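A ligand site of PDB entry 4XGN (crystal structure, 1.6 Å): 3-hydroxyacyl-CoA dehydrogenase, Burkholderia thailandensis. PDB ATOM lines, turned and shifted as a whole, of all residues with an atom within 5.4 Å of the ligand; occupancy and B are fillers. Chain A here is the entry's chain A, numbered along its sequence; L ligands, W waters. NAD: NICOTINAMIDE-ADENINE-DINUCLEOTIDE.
Water W9 bridges an oxygen (O3B) of the ligand (2.8 Å) and the side-chain amide nitrogen (ND2) of Asn 46 (2.9 Å).
Water W6 lies within hydrogen-bond range of O of Gly 93 and O1A of the ligand.
Water W2 lies within hydrogen-bond range of N of Gly 26 (2.8 Å), O of Gly 20 (2.9 Å), O2N of the ligand (2.9 Å) and O of Ser 23 (3.0 Å).
Water W8 bridges OG of Ser 153 and O of Gly 197.
N1A of the ligand lies close to O of Cys 64, at 3.4 Å.
CA of Gly 20 touches O4B of the ligand (3.5 Å).
CA of Gly 24 touches O2N of the ligand, 3.3 Å away.
Leu 45 touches the ligand (CD1 to C5A, 3.4 Å).
Ala 92 touches the ligand.
Gly 93 touches the ligand.
CG1 of Val 118 touches N6A of the ligand, at 3.7 Å.
CG2 of Thr 151 touches O4D of the ligand, at 3.4 Å.
Ala 152 touches the ligand (O to C6N, 3.4 Å).
Ser 153 touches the ligand (OG to C5N, 3.8 Å).
Pro 196 touches the ligand.
Gly 197 touches the ligand (O to C4N, 3.2 Å).
Ile 198 touches the ligand (CA to O7N, 3.5 Å).
Pro 202 touches the ligand.
CB of Met 203 touches O3 of the ligand (3.4 Å).
Hydrophobic or aromatic side chains within 4 Å of the ligand: Leu 25, Leu 45, Val 66, Ala 92, Val 118, Tyr 166, Pro 196, Phe 199, Pro 202 and Met 203.
Within 4 Å of the ligand: Gly 20, Ser 23, Gly 24, Leu 25, Asp 44, Leu 45, Cys 64, Asp 65, Val 66, Cys 91, Ala 92, Gly 93, Val 118, Thr 151, Ala 152, Ser 153, Tyr 166, Lys 170, Pro 196, Gly 197, Ile 198, Phe 199, Thr 201, Pro 202 and Met 203.
The nearest printed residue that does not touch the ligand is Ala 22 (4.1 Å).
O of Thr 151 sits at hydrogen-bond distance from NZ of Lys 170 (2.9 Å).
The backbone carbonyl oxygen of Pro 196 is in hydrogen-bond range of the backbone NH of Val 154.
SG of Cys 91 lies within hydrogen-bond range of OG1 of Thr 151 (3.7 Å).
The backbone NH (N) of Ala 67 sits at hydrogen-bond distance from the side-chain carboxylate (OD1) of Asp 65 (3.0 Å).
The side-chain amino group (NZ) of Lys 170 is in hydrogen-bond range of the backbone carbonyl oxygen (O) of Ala 152 (3.3 Å).
OD1 of Asp 44 is in hydrogen-bond range of N of Asn 46.
The backbone NH (N) of Gly 20 is in hydrogen-bond range of the backbone carbonyl oxygen (O) of Ala 43 (2.9 Å).
The side-chain carboxylate of Asp 44 is in hydrogen-bond range of the backbone NH of Ala 22 (3.0 Å).
OG1 of Thr 201 sits at hydrogen-bond distance from O1N of the ligand.
The backbone NH (N) of Val 66 sits at hydrogen-bond distance from a nitrogen (N1A) of the ligand, at 3.1 Å.
The backbone NH (N) of Phe 199 is in hydrogen-bond range of an oxygen (O7N) of the ligand, at 2.8 Å.
OG of Ser 23 sits at hydrogen-bond distance from O2A of the ligand (2.6 Å).
A nitrogen (N7N) of the ligand sits at hydrogen-bond distance from the backbone carbonyl oxygen (O) of Phe 199.
The backbone NH (N) of Leu 25 sits at hydrogen-bond distance from an oxygen (O2N) of the ligand (2.7 Å).
The backbone carbonyl oxygen of Cys 91 sits close to an oxygen (O3D) of the ligand (3.2 Å).
The side-chain carboxylate of Asp 65 is in hydrogen-bond range of a nitrogen (N6A) of the ligand (3.0 Å).
OD1 of Asp 44 sits at hydrogen-bond distance from O2B of the ligand, at 2.6 Å.
NZ of Lys 170 lies within hydrogen-bond range of O3D of the ligand.
An oxygen (O2D) of the ligand is in hydrogen-bond range of the side-chain hydroxyl (OH) of Tyr 166.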
ATOM      1  N   GLY A  20      18.102  -9.043  17.617  1.00  0.00           N
ATOM      2  CA  GLY A  20      17.159 -10.104  17.951  1.00  0.00           C
ATOM      3  C   GLY A  20      16.837 -10.143  19.436  1.00  0.00           C
ATOM      4  O   GLY A  20      16.359 -11.129  19.952  1.00  0.00           O
ATOM      5  N   GLY A  21      17.015  -9.005  20.100  1.00  0.00           N
ATOM      6  CA  GLY A  21      16.953  -8.973  21.532  1.00  0.00           C
ATOM      7  C   GLY A  21      15.523  -8.989  22.078  1.00  0.00           C
ATOM      8  O   GLY A  21      15.370  -9.091  23.281  1.00  0.00           O
ATOM      9  N   ALA A  22      14.498  -8.949  21.211  1.00  0.00           N
ATOM     10  CA  ALA A  22      13.124  -9.061  21.681  1.00  0.00           C
ATOM     11  C   ALA A  22      12.711 -10.485  22.077  1.00  0.00           C
ATOM     12  O   ALA A  22      11.662 -10.673  22.676  1.00  0.00           O
ATOM     13  CB  ALA A  22      12.143  -8.499  20.675  1.00  0.00           C
ATOM     14  N   SER A  23      13.500 -11.510  21.737  1.00  0.00           N
ATOM     15  CA  SER A  23      13.004 -12.903  21.855  1.00  0.00           C
ATOM     16  C   SER A  23      14.168 -13.855  22.054  1.00  0.00           C
ATOM     17  O   SER A  23      15.328 -13.497  21.805  1.00  0.00           O
ATOM     18  CB  SER A  23      12.279 -13.256  20.550  1.00  0.00           C
ATOM     19  OG  SER A  23      11.755 -14.564  20.430  1.00  0.00           O
ATOM     20  N   GLY A  24      13.832 -15.057  22.522  1.00  0.00           N
ATOM     21  CA  GLY A  24      14.708 -16.223  22.433  1.00  0.00           C
ATOM     22  C   GLY A  24      16.100 -15.968  22.985  1.00  0.00           C
ATOM     23  O   GLY A  24      16.283 -15.519  24.151  1.00  0.00           O
ATOM     24  N   LEU A  25      17.102 -16.298  22.167  1.00  0.00           N
ATOM     25  CA  LEU A  25      18.471 -16.180  22.636  1.00  0.00           C
ATOM     26  C   LEU A  25      18.914 -14.747  22.925  1.00  0.00           C
ATOM     27  O   LEU A  25      19.612 -14.516  23.912  1.00  0.00           O
ATOM     28  CB  LEU A  25      19.434 -16.877  21.657  1.00  0.00           C
ATOM     29  CG  LEU A  25      19.161 -18.298  21.300  1.00  0.00           C
ATOM     30  CD1 LEU A  25      20.277 -18.904  20.420  1.00  0.00           C
ATOM     31  CD2 LEU A  25      18.927 -19.177  22.544  1.00  0.00           C
ATOM     32  N   GLY A  26      18.485 -13.795  22.106  1.00  0.00           N
ATOM     33  CA  GLY A  26      18.786 -12.401  22.324  1.00  0.00           C
ATOM     34  C   GLY A  26      18.216 -11.898  23.643  1.00  0.00           C
ATOM     35  O   GLY A  26      18.921 -11.238  24.411  1.00  0.00           O
ATOM     36  N   ALA A  43      17.841  -4.390  19.730  1.00  0.00           N
ATOM     37  CA  ALA A  43      17.590  -4.043  18.324  1.00  0.00           C
ATOM     38  C   ALA A  43      16.812  -5.185  17.664  1.00  0.00           C
ATOM     39  O   ALA A  43      17.265  -6.313  17.623  1.00  0.00           O
ATOM     40  CB  ALA A  43      18.913  -3.776  17.637  1.00  0.00           C
ATOM     41  N   ASP A  44      15.582  -4.944  17.224  1.00  0.00           N
ATOM     42  CA  ASP A  44      14.751  -5.995  16.710  1.00  0.00           C
ATOM     43  C   ASP A  44      13.679  -5.402  15.835  1.00  0.00           C
ATOM     44  O   ASP A  44      13.394  -4.198  15.940  1.00  0.00           O
ATOM     45  CB  ASP A  44      14.089  -6.728  17.909  1.00  0.00           C
ATOM     46  CG  ASP A  44      13.638  -8.150  17.581  1.00  0.00           C
ATOM     47  OD1 ASP A  44      12.687  -8.338  16.792  1.00  0.00           O
ATOM     48  OD2 ASP A  44      14.234  -9.101  18.188  1.00  0.00           O
ATOM     49  N   LEU A  45      13.059  -6.246  15.003  1.00  0.00           N
ATOM     50  CA  LEU A  45      11.830  -5.848  14.300  1.00  0.00           C
ATOM     51  C   LEU A  45      10.586  -5.725  15.209  1.00  0.00           C
ATOM     52  O   LEU A  45       9.628  -4.984  14.870  1.00  0.00           O
ATOM     53  CB  LEU A  45      11.529  -6.848  13.182  1.00  0.00           C
ATOM     54  CG  LEU A  45      12.656  -7.097  12.194  1.00  0.00           C
ATOM     55  CD1 LEU A  45      12.252  -8.253  11.280  1.00  0.00           C
ATOM     56  CD2 LEU A  45      12.961  -5.823  11.411  1.00  0.00           C
ATOM     57  N   ASN A  46      10.583  -6.468  16.325  1.00  0.00           N
ATOM     58  CA  ASN A  46       9.381  -6.649  17.101  1.00  0.00           C
ATOM     59  C   ASN A  46       9.241  -5.472  18.057  1.00  0.00           C
ATOM     60  O   ASN A  46       9.877  -5.468  19.105  1.00  0.00           O
ATOM     61  CB  ASN A  46       9.437  -7.955  17.890  1.00  0.00           C
ATOM     62  CG  ASN A  46       8.125  -8.304  18.540  1.00  0.00           C
ATOM     63  OD1 ASN A  46       7.333  -7.437  18.897  1.00  0.00           O
ATOM     64  ND2 ASN A  46       7.920  -9.602  18.785  1.00  0.00           N
ATOM     65  N   CYS A  64      14.959  -1.978  14.607  1.00  0.00           N
ATOM     66  CA  CYS A  64      16.150  -2.119  13.793  1.00  0.00           C
ATOM     67  C   CYS A  64      16.078  -3.357  12.934  1.00  0.00           C
ATOM     68  O   CYS A  64      16.005  -4.478  13.434  1.00  0.00           O
ATOM     69  CB  CYS A  64      17.380  -2.074  14.708  1.00  0.00           C
ATOM     70  SG  CYS A  64      18.943  -2.537  13.887  1.00  0.00           S
ATOM     71  N   ASP A  65      15.989  -3.137  11.630  1.00  0.00           N
ATOM     72  CA  ASP A  65      16.179  -4.215  10.660  1.00  0.00           C
ATOM     73  C   ASP A  65      17.635  -4.256  10.402  1.00  0.00           C
ATOM     74  O   ASP A  65      18.202  -3.320   9.850  1.00  0.00           O
ATOM     75  CB  ASP A  65      15.417  -3.921   9.386  1.00  0.00           C
ATOM     76  CG  ASP A  65      15.461  -5.061   8.367  1.00  0.00           C
ATOM     77  OD1 ASP A  65      16.430  -5.897   8.383  1.00  0.00           O
ATOM     78  OD2 ASP A  65      14.512  -5.061   7.508  1.00  0.00           O
ATOM     79  N   VAL A  66      18.269  -5.344  10.820  1.00  0.00           N
ATOM     80  CA  VAL A  66      19.718  -5.443  10.730  1.00  0.00           C
ATOM     81  C   VAL A  66      20.272  -5.363   9.308  1.00  0.00           C
ATOM     82  O   VAL A  66      21.464  -5.087   9.146  1.00  0.00           O
ATOM     83  CB  VAL A  66      20.274  -6.751  11.404  1.00  0.00           C
ATOM     84  CG1 VAL A  66      20.002  -6.751  12.900  1.00  0.00           C
ATOM     85  CG2 VAL A  66      19.726  -7.993  10.731  1.00  0.00           C
ATOM     86  N   ALA A  67      19.435  -5.559   8.302  1.00  0.00           N
ATOM     87  CA  ALA A  67      19.857  -5.405   6.917  1.00  0.00           C
ATOM     88  C   ALA A  67      19.957  -3.981   6.427  1.00  0.00           C
ATOM     89  O   ALA A  67      20.442  -3.760   5.309  1.00  0.00           O
ATOM     90  CB  ALA A  67      18.992  -6.239   5.971  1.00  0.00           C
ATOM     91  N   ASN A  90      25.039 -10.495  18.114  1.00  0.00           N
ATOM     92  CA  ASN A  90      24.180 -10.675  16.936  1.00  0.00           C
ATOM     93  C   ASN A  90      23.321 -11.923  17.088  1.00  0.00           C
ATOM     94  O   ASN A  90      23.841 -13.025  16.917  1.00  0.00           O
ATOM     95  CB  ASN A  90      25.000 -10.785  15.664  1.00  0.00           C
ATOM     96  CG  ASN A  90      25.707  -9.512  15.303  1.00  0.00           C
ATOM     97  OD1 ASN A  90      25.068  -8.524  14.983  1.00  0.00           O
ATOM     98  ND2 ASN A  90      27.018  -9.496  15.402  1.00  0.00           N
ATOM     99  N   CYS A  91      22.054 -11.751  17.435  1.00  0.00           N
ATOM    100  CA  CYS A  91      21.094 -12.856  17.479  1.00  0.00           C
ATOM    101  C   CYS A  91      19.935 -12.757  16.466  1.00  0.00           C
ATOM    102  O   CYS A  91      19.240 -13.742  16.284  1.00  0.00           O
ATOM    103  CB  CYS A  91      20.513 -13.036  18.875  1.00  0.00           C
ATOM    104  SG  CYS A  91      21.724 -13.507  20.124  1.00  0.00           S
ATOM    105  N   ALA A  92      19.760 -11.640  15.774  1.00  0.00           N
ATOM    106  CA  ALA A  92      18.751 -11.524  14.748  1.00  0.00           C
ATOM    107  C   ALA A  92      18.978 -12.580  13.654  1.00  0.00           C
ATOM    108  O   ALA A  92      20.061 -12.675  13.111  1.00  0.00           O
ATOM    109  CB  ALA A  92      18.779 -10.166  14.109  1.00  0.00           C
ATOM    110  N   GLY A  93      17.954 -13.369  13.375  1.00  0.00           N
ATOM    111  CA  GLY A  93      18.072 -14.401  12.365  1.00  0.00           C
ATOM    112  C   GLY A  93      16.732 -15.035  12.105  1.00  0.00           C
ATOM    113  O   GLY A  93      15.820 -14.905  12.931  1.00  0.00           O
ATOM    114  N   ILE A  94      16.628 -15.698  10.931  1.00  0.00           N
ATOM    115  CA  ILE A  94      15.476 -16.459  10.522  1.00  0.00           C
ATOM    116  C   ILE A  94      16.002 -17.808   9.990  1.00  0.00           C
ATOM    117  O   ILE A  94      17.156 -17.899   9.563  1.00  0.00           O
ATOM    118  CB  ILE A  94      14.649 -15.764   9.415  1.00  0.00           C
ATOM    119  CG1 ILE A  94      15.535 -15.309   8.256  1.00  0.00           C
ATOM    120  CG2 ILE A  94      13.927 -14.557   9.982  1.00  0.00           C
ATOM    121  CD1 ILE A  94      14.787 -14.784   7.060  1.00  0.00           C
ATOM    122  N   ALA A  95      15.142 -18.832  10.069  1.00  0.00           N
ATOM    123  CA  ALA A  95      15.529 -20.202   9.662  1.00  0.00           C
ATOM    124  C   ALA A  95      14.435 -20.874   8.823  1.00  0.00           C
ATOM    125  O   ALA A  95      13.845 -21.862   9.222  1.00  0.00           O
ATOM    126  CB  ALA A  95      15.856 -21.046  10.868  1.00  0.00           C
ATOM    127  N   VAL A 118      19.282 -11.407   5.944  1.00  0.00           N
ATOM    128  CA  VAL A 118      19.099 -11.198   7.350  1.00  0.00           C
ATOM    129  C   VAL A 118      20.248 -11.738   8.167  1.00  0.00           C
ATOM    130  O   VAL A 118      20.783 -11.054   9.022  1.00  0.00           O
ATOM    131  CB  VAL A 118      17.781 -11.796   7.850  1.00  0.00           C
ATOM    132  CG1 VAL A 118      17.642 -11.683   9.345  1.00  0.00           C
ATOM    133  CG2 VAL A 118      16.628 -11.101   7.144  1.00  0.00           C
ATOM    134  N   ASN A 119      20.622 -13.003   7.903  1.00  0.00           N
ATOM    135  CA  ASN A 119      21.512 -13.713   8.788  1.00  0.00           C
ATOM    136  C   ASN A 119      22.960 -13.347   8.619  1.00  0.00           C
ATOM    137  O   ASN A 119      23.694 -13.328   9.596  1.00  0.00           O
ATOM    138  CB  ASN A 119      21.355 -15.219   8.580  1.00  0.00           C
ATOM    139  CG  ASN A 119      20.015 -15.763   9.046  1.00  0.00           C
ATOM    140  OD1 ASN A 119      19.151 -15.031   9.567  1.00  0.00           O
ATOM    141  ND2 ASN A 119      19.843 -17.075   8.902  1.00  0.00           N
ATOM    142  N   THR A 151      26.023 -15.197  16.150  1.00  0.00           N
ATOM    143  CA  THR A 151      25.388 -16.489  16.273  1.00  0.00           C
ATOM    144  C   THR A 151      25.364 -17.169  14.920  1.00  0.00           C
ATOM    145  O   THR A 151      24.726 -16.688  13.967  1.00  0.00           O
ATOM    146  CB  THR A 151      23.950 -16.385  16.830  1.00  0.00           C
ATOM    147  OG1 THR A 151      23.934 -15.510  17.998  1.00  0.00           O
ATOM    148  CG2 THR A 151      23.434 -17.760  17.184  1.00  0.00           C
ATOM    149  N   ALA A 152      26.084 -18.263  14.790  1.00  0.00           N
ATOM    150  CA  ALA A 152      25.973 -19.104  13.670  1.00  0.00           C
ATOM    151  C   ALA A 152      24.902 -20.193  14.017  1.00  0.00           C
ATOM    152  O   ALA A 152      23.783 -19.839  14.361  1.00  0.00           O
ATOM    153  CB  ALA A 152      27.323 -19.667  13.262  1.00  0.00           C
ATOM    154  N   SER A 153      25.241 -21.468  13.895  1.00  0.00           N
ATOM    155  CA  SER A 153      24.370 -22.644  14.125  1.00  0.00           C
ATOM    156  C   SER A 153      25.239 -23.835  13.814  1.00  0.00           C
ATOM    157  O   SER A 153      26.180 -23.727  13.033  1.00  0.00           O
ATOM    158  CB  SER A 153      23.206 -22.672  13.135  1.00  0.00           C
ATOM    159  OG  SER A 153      22.503 -23.894  13.197  1.00  0.00           O
ATOM    160  N   VAL A 154      24.872 -24.981  14.367  1.00  0.00           N
ATOM    161  CA  VAL A 154      25.463 -26.237  13.955  1.00  0.00           C
ATOM    162  C   VAL A 154      25.139 -26.510  12.476  1.00  0.00           C
ATOM    163  O   VAL A 154      25.859 -27.251  11.831  1.00  0.00           O
ATOM    164  CB  VAL A 154      25.050 -27.417  14.861  1.00  0.00           C
ATOM    165  CG1 VAL A 154      25.552 -27.203  16.278  1.00  0.00           C
ATOM    166  CG2 VAL A 154      23.561 -27.711  14.776  1.00  0.00           C
ATOM    167  N   TYR A 166      19.878 -21.569   5.144  1.00  0.00           N
ATOM    168  CA  TYR A 166      20.260 -21.335   6.530  1.00  0.00           C
ATOM    169  C   TYR A 166      21.714 -21.748   6.777  1.00  0.00           C
ATOM    170  O   TYR A 166      22.498 -20.975   7.299  1.00  0.00           O
ATOM    171  CB  TYR A 166      19.335 -22.118   7.434  1.00  0.00           C
ATOM    172  CG  TYR A 166      19.502 -21.823   8.902  1.00  0.00           C
ATOM    173  CD1 TYR A 166      19.169 -20.599   9.425  1.00  0.00           C
ATOM    174  CD2 TYR A 166      19.892 -22.812   9.768  1.00  0.00           C
ATOM    175  CE1 TYR A 166      19.267 -20.340  10.772  1.00  0.00           C
ATOM    176  CE2 TYR A 166      20.014 -22.570  11.124  1.00  0.00           C
ATOM    177  CZ  TYR A 166      19.657 -21.337  11.634  1.00  0.00           C
ATOM    178  OH  TYR A 166      19.723 -21.050  12.992  1.00  0.00           O
ATOM    179  N   LYS A 170      24.801 -19.308   7.895  1.00  0.00           N
ATOM    180  CA  LYS A 170      25.473 -19.505   9.161  1.00  0.00           C
ATOM    181  C   LYS A 170      26.945 -19.927   8.991  1.00  0.00           C
ATOM    182  O   LYS A 170      27.801 -19.566   9.781  1.00  0.00           O
ATOM    183  CB  LYS A 170      24.676 -20.495  10.003  1.00  0.00           C
ATOM    184  CG  LYS A 170      23.292 -20.013  10.350  1.00  0.00           C
ATOM    185  CD  LYS A 170      23.304 -18.694  11.024  1.00  0.00           C
ATOM    186  CE  LYS A 170      22.026 -18.458  11.793  1.00  0.00           C
ATOM    187  NZ  LYS A 170      22.157 -17.389  12.790  1.00  0.00           N
ATOM    188  N   PRO A 196      24.993 -22.537  18.046  1.00  0.00           N
ATOM    189  CA  PRO A 196      24.095 -23.357  18.853  1.00  0.00           C
ATOM    190  C   PRO A 196      23.524 -24.567  18.122  1.00  0.00           C
ATOM    191  O   PRO A 196      23.393 -24.564  16.881  1.00  0.00           O
ATOM    192  CB  PRO A 196      22.965 -22.374  19.258  1.00  0.00           C
ATOM    193  CG  PRO A 196      23.465 -21.012  18.866  1.00  0.00           C
ATOM    194  CD  PRO A 196      24.434 -21.195  17.764  1.00  0.00           C
ATOM    195  N   GLY A 197      23.197 -25.603  18.890  1.00  0.00           N
ATOM    196  CA  GLY A 197      22.484 -26.743  18.369  1.00  0.00           C
ATOM    197  C   GLY A 197      20.981 -26.509  18.279  1.00  0.00           C
ATOM    198  O   GLY A 197      20.501 -25.978  17.271  1.00  0.00           O
ATOM    199  N   ILE A 198      20.231 -26.973  19.285  1.00  0.00           N
ATOM    200  CA  ILE A 198      18.782 -26.782  19.252  1.00  0.00           C
ATOM    201  C   ILE A 198      18.374 -26.223  20.588  1.00  0.00           C
ATOM    202  O   ILE A 198      18.623 -26.858  21.625  1.00  0.00           O
ATOM    203  CB  ILE A 198      17.981 -28.062  18.965  1.00  0.00           C
ATOM    204  CG1 ILE A 198      18.647 -28.892  17.863  1.00  0.00           C
ATOM    205  CG2 ILE A 198      16.547 -27.682  18.590  1.00  0.00           C
ATOM    206  CD1 ILE A 198      18.233 -30.332  17.959  1.00  0.00           C
ATOM    207  N   PHE A 199      17.728 -25.052  20.535  1.00  0.00           N
ATOM    208  CA  PHE A 199      17.365 -24.288  21.707  1.00  0.00           C
ATOM    209  C   PHE A 199      15.882 -24.014  21.750  1.00  0.00           C
ATOM    210  O   PHE A 199      15.275 -23.737  20.711  1.00  0.00           O
ATOM    211  CB  PHE A 199      18.168 -22.967  21.794  1.00  0.00           C
ATOM    212  CG  PHE A 199      19.506 -23.146  22.408  1.00  0.00           C
ATOM    213  CD1 PHE A 199      20.523 -23.841  21.734  1.00  0.00           C
ATOM    214  CD2 PHE A 199      19.754 -22.703  23.708  1.00  0.00           C
ATOM    215  CE1 PHE A 199      21.755 -24.043  22.311  1.00  0.00           C
ATOM    216  CE2 PHE A 199      20.981 -22.896  24.268  1.00  0.00           C
ATOM    217  CZ  PHE A 199      21.977 -23.561  23.603  1.00  0.00           C
ATOM    218  N   GLU A 200      15.338 -24.064  22.953  1.00  0.00           N
ATOM    219  CA  GLU A 200      13.925 -23.779  23.162  1.00  0.00           C
ATOM    220  C   GLU A 200      13.588 -22.268  23.064  1.00  0.00           C
ATOM    221  O   GLU A 200      13.713 -21.531  24.042  1.00  0.00           O
ATOM    222  CB  GLU A 200      13.477 -24.341  24.501  1.00  0.00           C
ATOM    223  CG  GLU A 200      11.979 -24.278  24.700  1.00  0.00           C
ATOM    224  CD  GLU A 200      11.588 -24.848  26.010  1.00  0.00           C
ATOM    225  OE1 GLU A 200      11.738 -24.141  27.000  1.00  0.00           O
ATOM    226  OE2 GLU A 200      11.172 -26.007  26.053  1.00  0.00           O
ATOM    227  N   THR A 201      13.165 -21.832  21.875  1.00  0.00           N
ATOM    228  CA  THR A 201      12.793 -20.455  21.628  1.00  0.00           C
ATOM    229  C   THR A 201      11.607 -20.405  20.664  1.00  0.00           C
ATOM    230  O   THR A 201      11.308 -21.383  20.023  1.00  0.00           O
ATOM    231  CB  THR A 201      13.957 -19.677  20.971  1.00  0.00           C
ATOM    232  OG1 THR A 201      14.135 -20.112  19.604  1.00  0.00           O
ATOM    233  CG2 THR A 201      15.229 -19.845  21.734  1.00  0.00           C
ATOM    234  N   PRO A 202      11.032 -19.216  20.452  1.00  0.00           N
ATOM    235  CA  PRO A 202      10.029 -19.116  19.393  1.00  0.00           C
ATOM    236  C   PRO A 202      10.494 -19.455  17.967  1.00  0.00           C
ATOM    237  O   PRO A 202       9.650 -19.653  17.090  1.00  0.00           O
ATOM    238  CB  PRO A 202       9.569 -17.646  19.498  1.00  0.00           C
ATOM    239  CG  PRO A 202       9.911 -17.242  20.906  1.00  0.00           C
ATOM    240  CD  PRO A 202      11.159 -17.965  21.225  1.00  0.00           C
ATOM    241  N   MET A 203      11.802 -19.570  17.702  1.00  0.00           N
ATOM    242  CA  MET A 203      12.230 -20.075  16.391  1.00  0.00           C
ATOM    243  C   MET A 203      11.610 -21.424  16.059  1.00  0.00           C
ATOM    244  O   MET A 203      11.422 -21.733  14.868  1.00  0.00           O
ATOM    245  CB  MET A 203      13.756 -20.163  16.278  1.00  0.00           C
ATOM    246  CG  MET A 203      14.216 -20.530  14.862  1.00  0.00           C
ATOM    247  SD  MET A 203      15.913 -20.112  14.572  1.00  0.00           S
ATOM    248  CE  MET A 203      15.716 -18.454  13.895  1.00  0.00           C
ATOM    249  N   LEU A 204      11.301 -22.239  17.087  1.00  0.00           N
ATOM    250  CA  LEU A 204      10.685 -23.551  16.915  1.00  0.00           C
ATOM    251  C   LEU A 204       9.138 -23.511  16.889  1.00  0.00           C
ATOM    252  O   LEU A 204       8.517 -24.570  16.860  1.00  0.00           O
ATOM    253  CB  LEU A 204      11.136 -24.519  18.012  1.00  0.00           C
ATOM    254  CG  LEU A 204      12.646 -24.605  18.266  1.00  0.00           C
ATOM    255  CD1 LEU A 204      12.927 -25.711  19.267  1.00  0.00           C
ATOM    256  CD2 LEU A 204      13.477 -24.795  17.016  1.00  0.00           C
HETATM  257  PA  NAD L   1      13.776 -16.034  17.779  1.00  0.00           P
HETATM  258  O1A NAD L   1      12.906 -16.133  16.579  1.00  0.00           O
HETATM  259  O2A NAD L   1      13.141 -16.295  19.118  1.00  0.00           O
HETATM  260  O5B NAD L   1      14.496 -14.601  17.855  1.00  0.00           O
HETATM  261  C5B NAD L   1      15.012 -13.989  16.691  1.00  0.00           C
HETATM  262  C4B NAD L   1      14.802 -12.474  16.789  1.00  0.00           C
HETATM  263  O4B NAD L   1      15.313 -12.029  15.638  1.00  0.00           O
HETATM  264  C3B NAD L   1      13.289 -12.104  16.764  1.00  0.00           C
HETATM  265  O3B NAD L   1      12.867 -11.373  17.873  1.00  0.00           O
HETATM  266  C2B NAD L   1      13.230 -11.385  15.405  1.00  0.00           C
HETATM  267  O2B NAD L   1      12.086 -10.462  15.360  1.00  0.00           O
HETATM  268  C1B NAD L   1      14.435 -10.869  15.199  1.00  0.00           C
HETATM  269  N9A NAD L   1      14.717 -10.631  13.810  1.00  0.00           N
HETATM  270  C8A NAD L   1      14.442 -11.413  12.713  1.00  0.00           C
HETATM  271  N7A NAD L   1      14.815 -10.755  11.572  1.00  0.00           N
HETATM  272  C5A NAD L   1      15.337  -9.606  12.001  1.00  0.00           C
HETATM  273  C6A NAD L   1      15.892  -8.570  11.310  1.00  0.00           C
HETATM  274  N6A NAD L   1      16.011  -8.396   9.897  1.00  0.00           N
HETATM  275  N1A NAD L   1      16.355  -7.514  11.991  1.00  0.00           N
HETATM  276  C2A NAD L   1      16.289  -7.448  13.361  1.00  0.00           C
HETATM  277  N3A NAD L   1      15.756  -8.496  14.053  1.00  0.00           N
HETATM  278  C4A NAD L   1      15.277  -9.538  13.347  1.00  0.00           C
HETATM  279  O3  NAD L   1      14.873 -17.158  17.466  1.00  0.00           O
HETATM  280  PN  NAD L   1      16.198 -17.455  18.355  1.00  0.00           P
HETATM  281  O1N NAD L   1      16.183 -18.932  18.609  1.00  0.00           O
HETATM  282  O2N NAD L   1      16.363 -16.607  19.607  1.00  0.00           O
HETATM  283  O5D NAD L   1      17.391 -17.126  17.313  1.00  0.00           O
HETATM  284  C5D NAD L   1      18.535 -16.364  17.677  1.00  0.00           C
HETATM  285  C4D NAD L   1      19.725 -16.666  16.844  1.00  0.00           C
HETATM  286  O4D NAD L   1      20.074 -17.949  17.171  1.00  0.00           O
HETATM  287  C3D NAD L   1      19.403 -16.677  15.324  1.00  0.00           C
HETATM  288  O3D NAD L   1      20.444 -16.195  14.588  1.00  0.00           O
HETATM  289  C2D NAD L   1      19.184 -18.200  15.109  1.00  0.00           C
HETATM  290  O2D NAD L   1      19.300 -18.555  13.660  1.00  0.00           O
HETATM  291  C1D NAD L   1      20.125 -18.755  15.836  1.00  0.00           C
HETATM  292  N1N NAD L   1      19.976 -20.151  16.236  1.00  0.00           N
HETATM  293  C2N NAD L   1      18.872 -20.638  16.902  1.00  0.00           C
HETATM  294  C3N NAD L   1      18.763 -21.971  17.269  1.00  0.00           C
HETATM  295  C7N NAD L   1      17.555 -22.543  17.946  1.00  0.00           C
HETATM  296  O7N NAD L   1      17.435 -23.750  18.024  1.00  0.00           O
HETATM  297  N7N NAD L   1      16.583 -21.692  18.545  1.00  0.00           N
HETATM  298  C4N NAD L   1      19.840 -22.837  16.964  1.00  0.00           C
HETATM  299  C5N NAD L   1      20.950 -22.346  16.333  1.00  0.00           C
HETATM  300  C6N NAD L   1      21.032 -21.012  15.985  1.00  0.00           C
HETATM  301  O   HOH W   1      21.974 -14.007  14.470  1.00  0.00           O
HETATM  302  O   HOH W   2      17.253 -13.831  19.541  1.00  0.00           O
HETATM  303  O   HOH W   3      13.295 -11.195   9.150  1.00  0.00           O
HETATM  304  O   HOH W   4       9.891 -10.261  13.844  1.00  0.00           O
HETATM  305  O   HOH W   5      10.323 -15.532  16.376  1.00  0.00           O
HETATM  306  O   HOH W   6      13.350 -15.881  13.714  1.00  0.00           O
HETATM  307  O   HOH W   7      11.933 -13.712  12.955  1.00  0.00           O
HETATM  308  O   HOH W   8      20.717 -25.248  14.665  1.00  0.00           O
HETATM  309  O   HOH W   9      10.033 -11.469  17.945  1.00  0.00           O
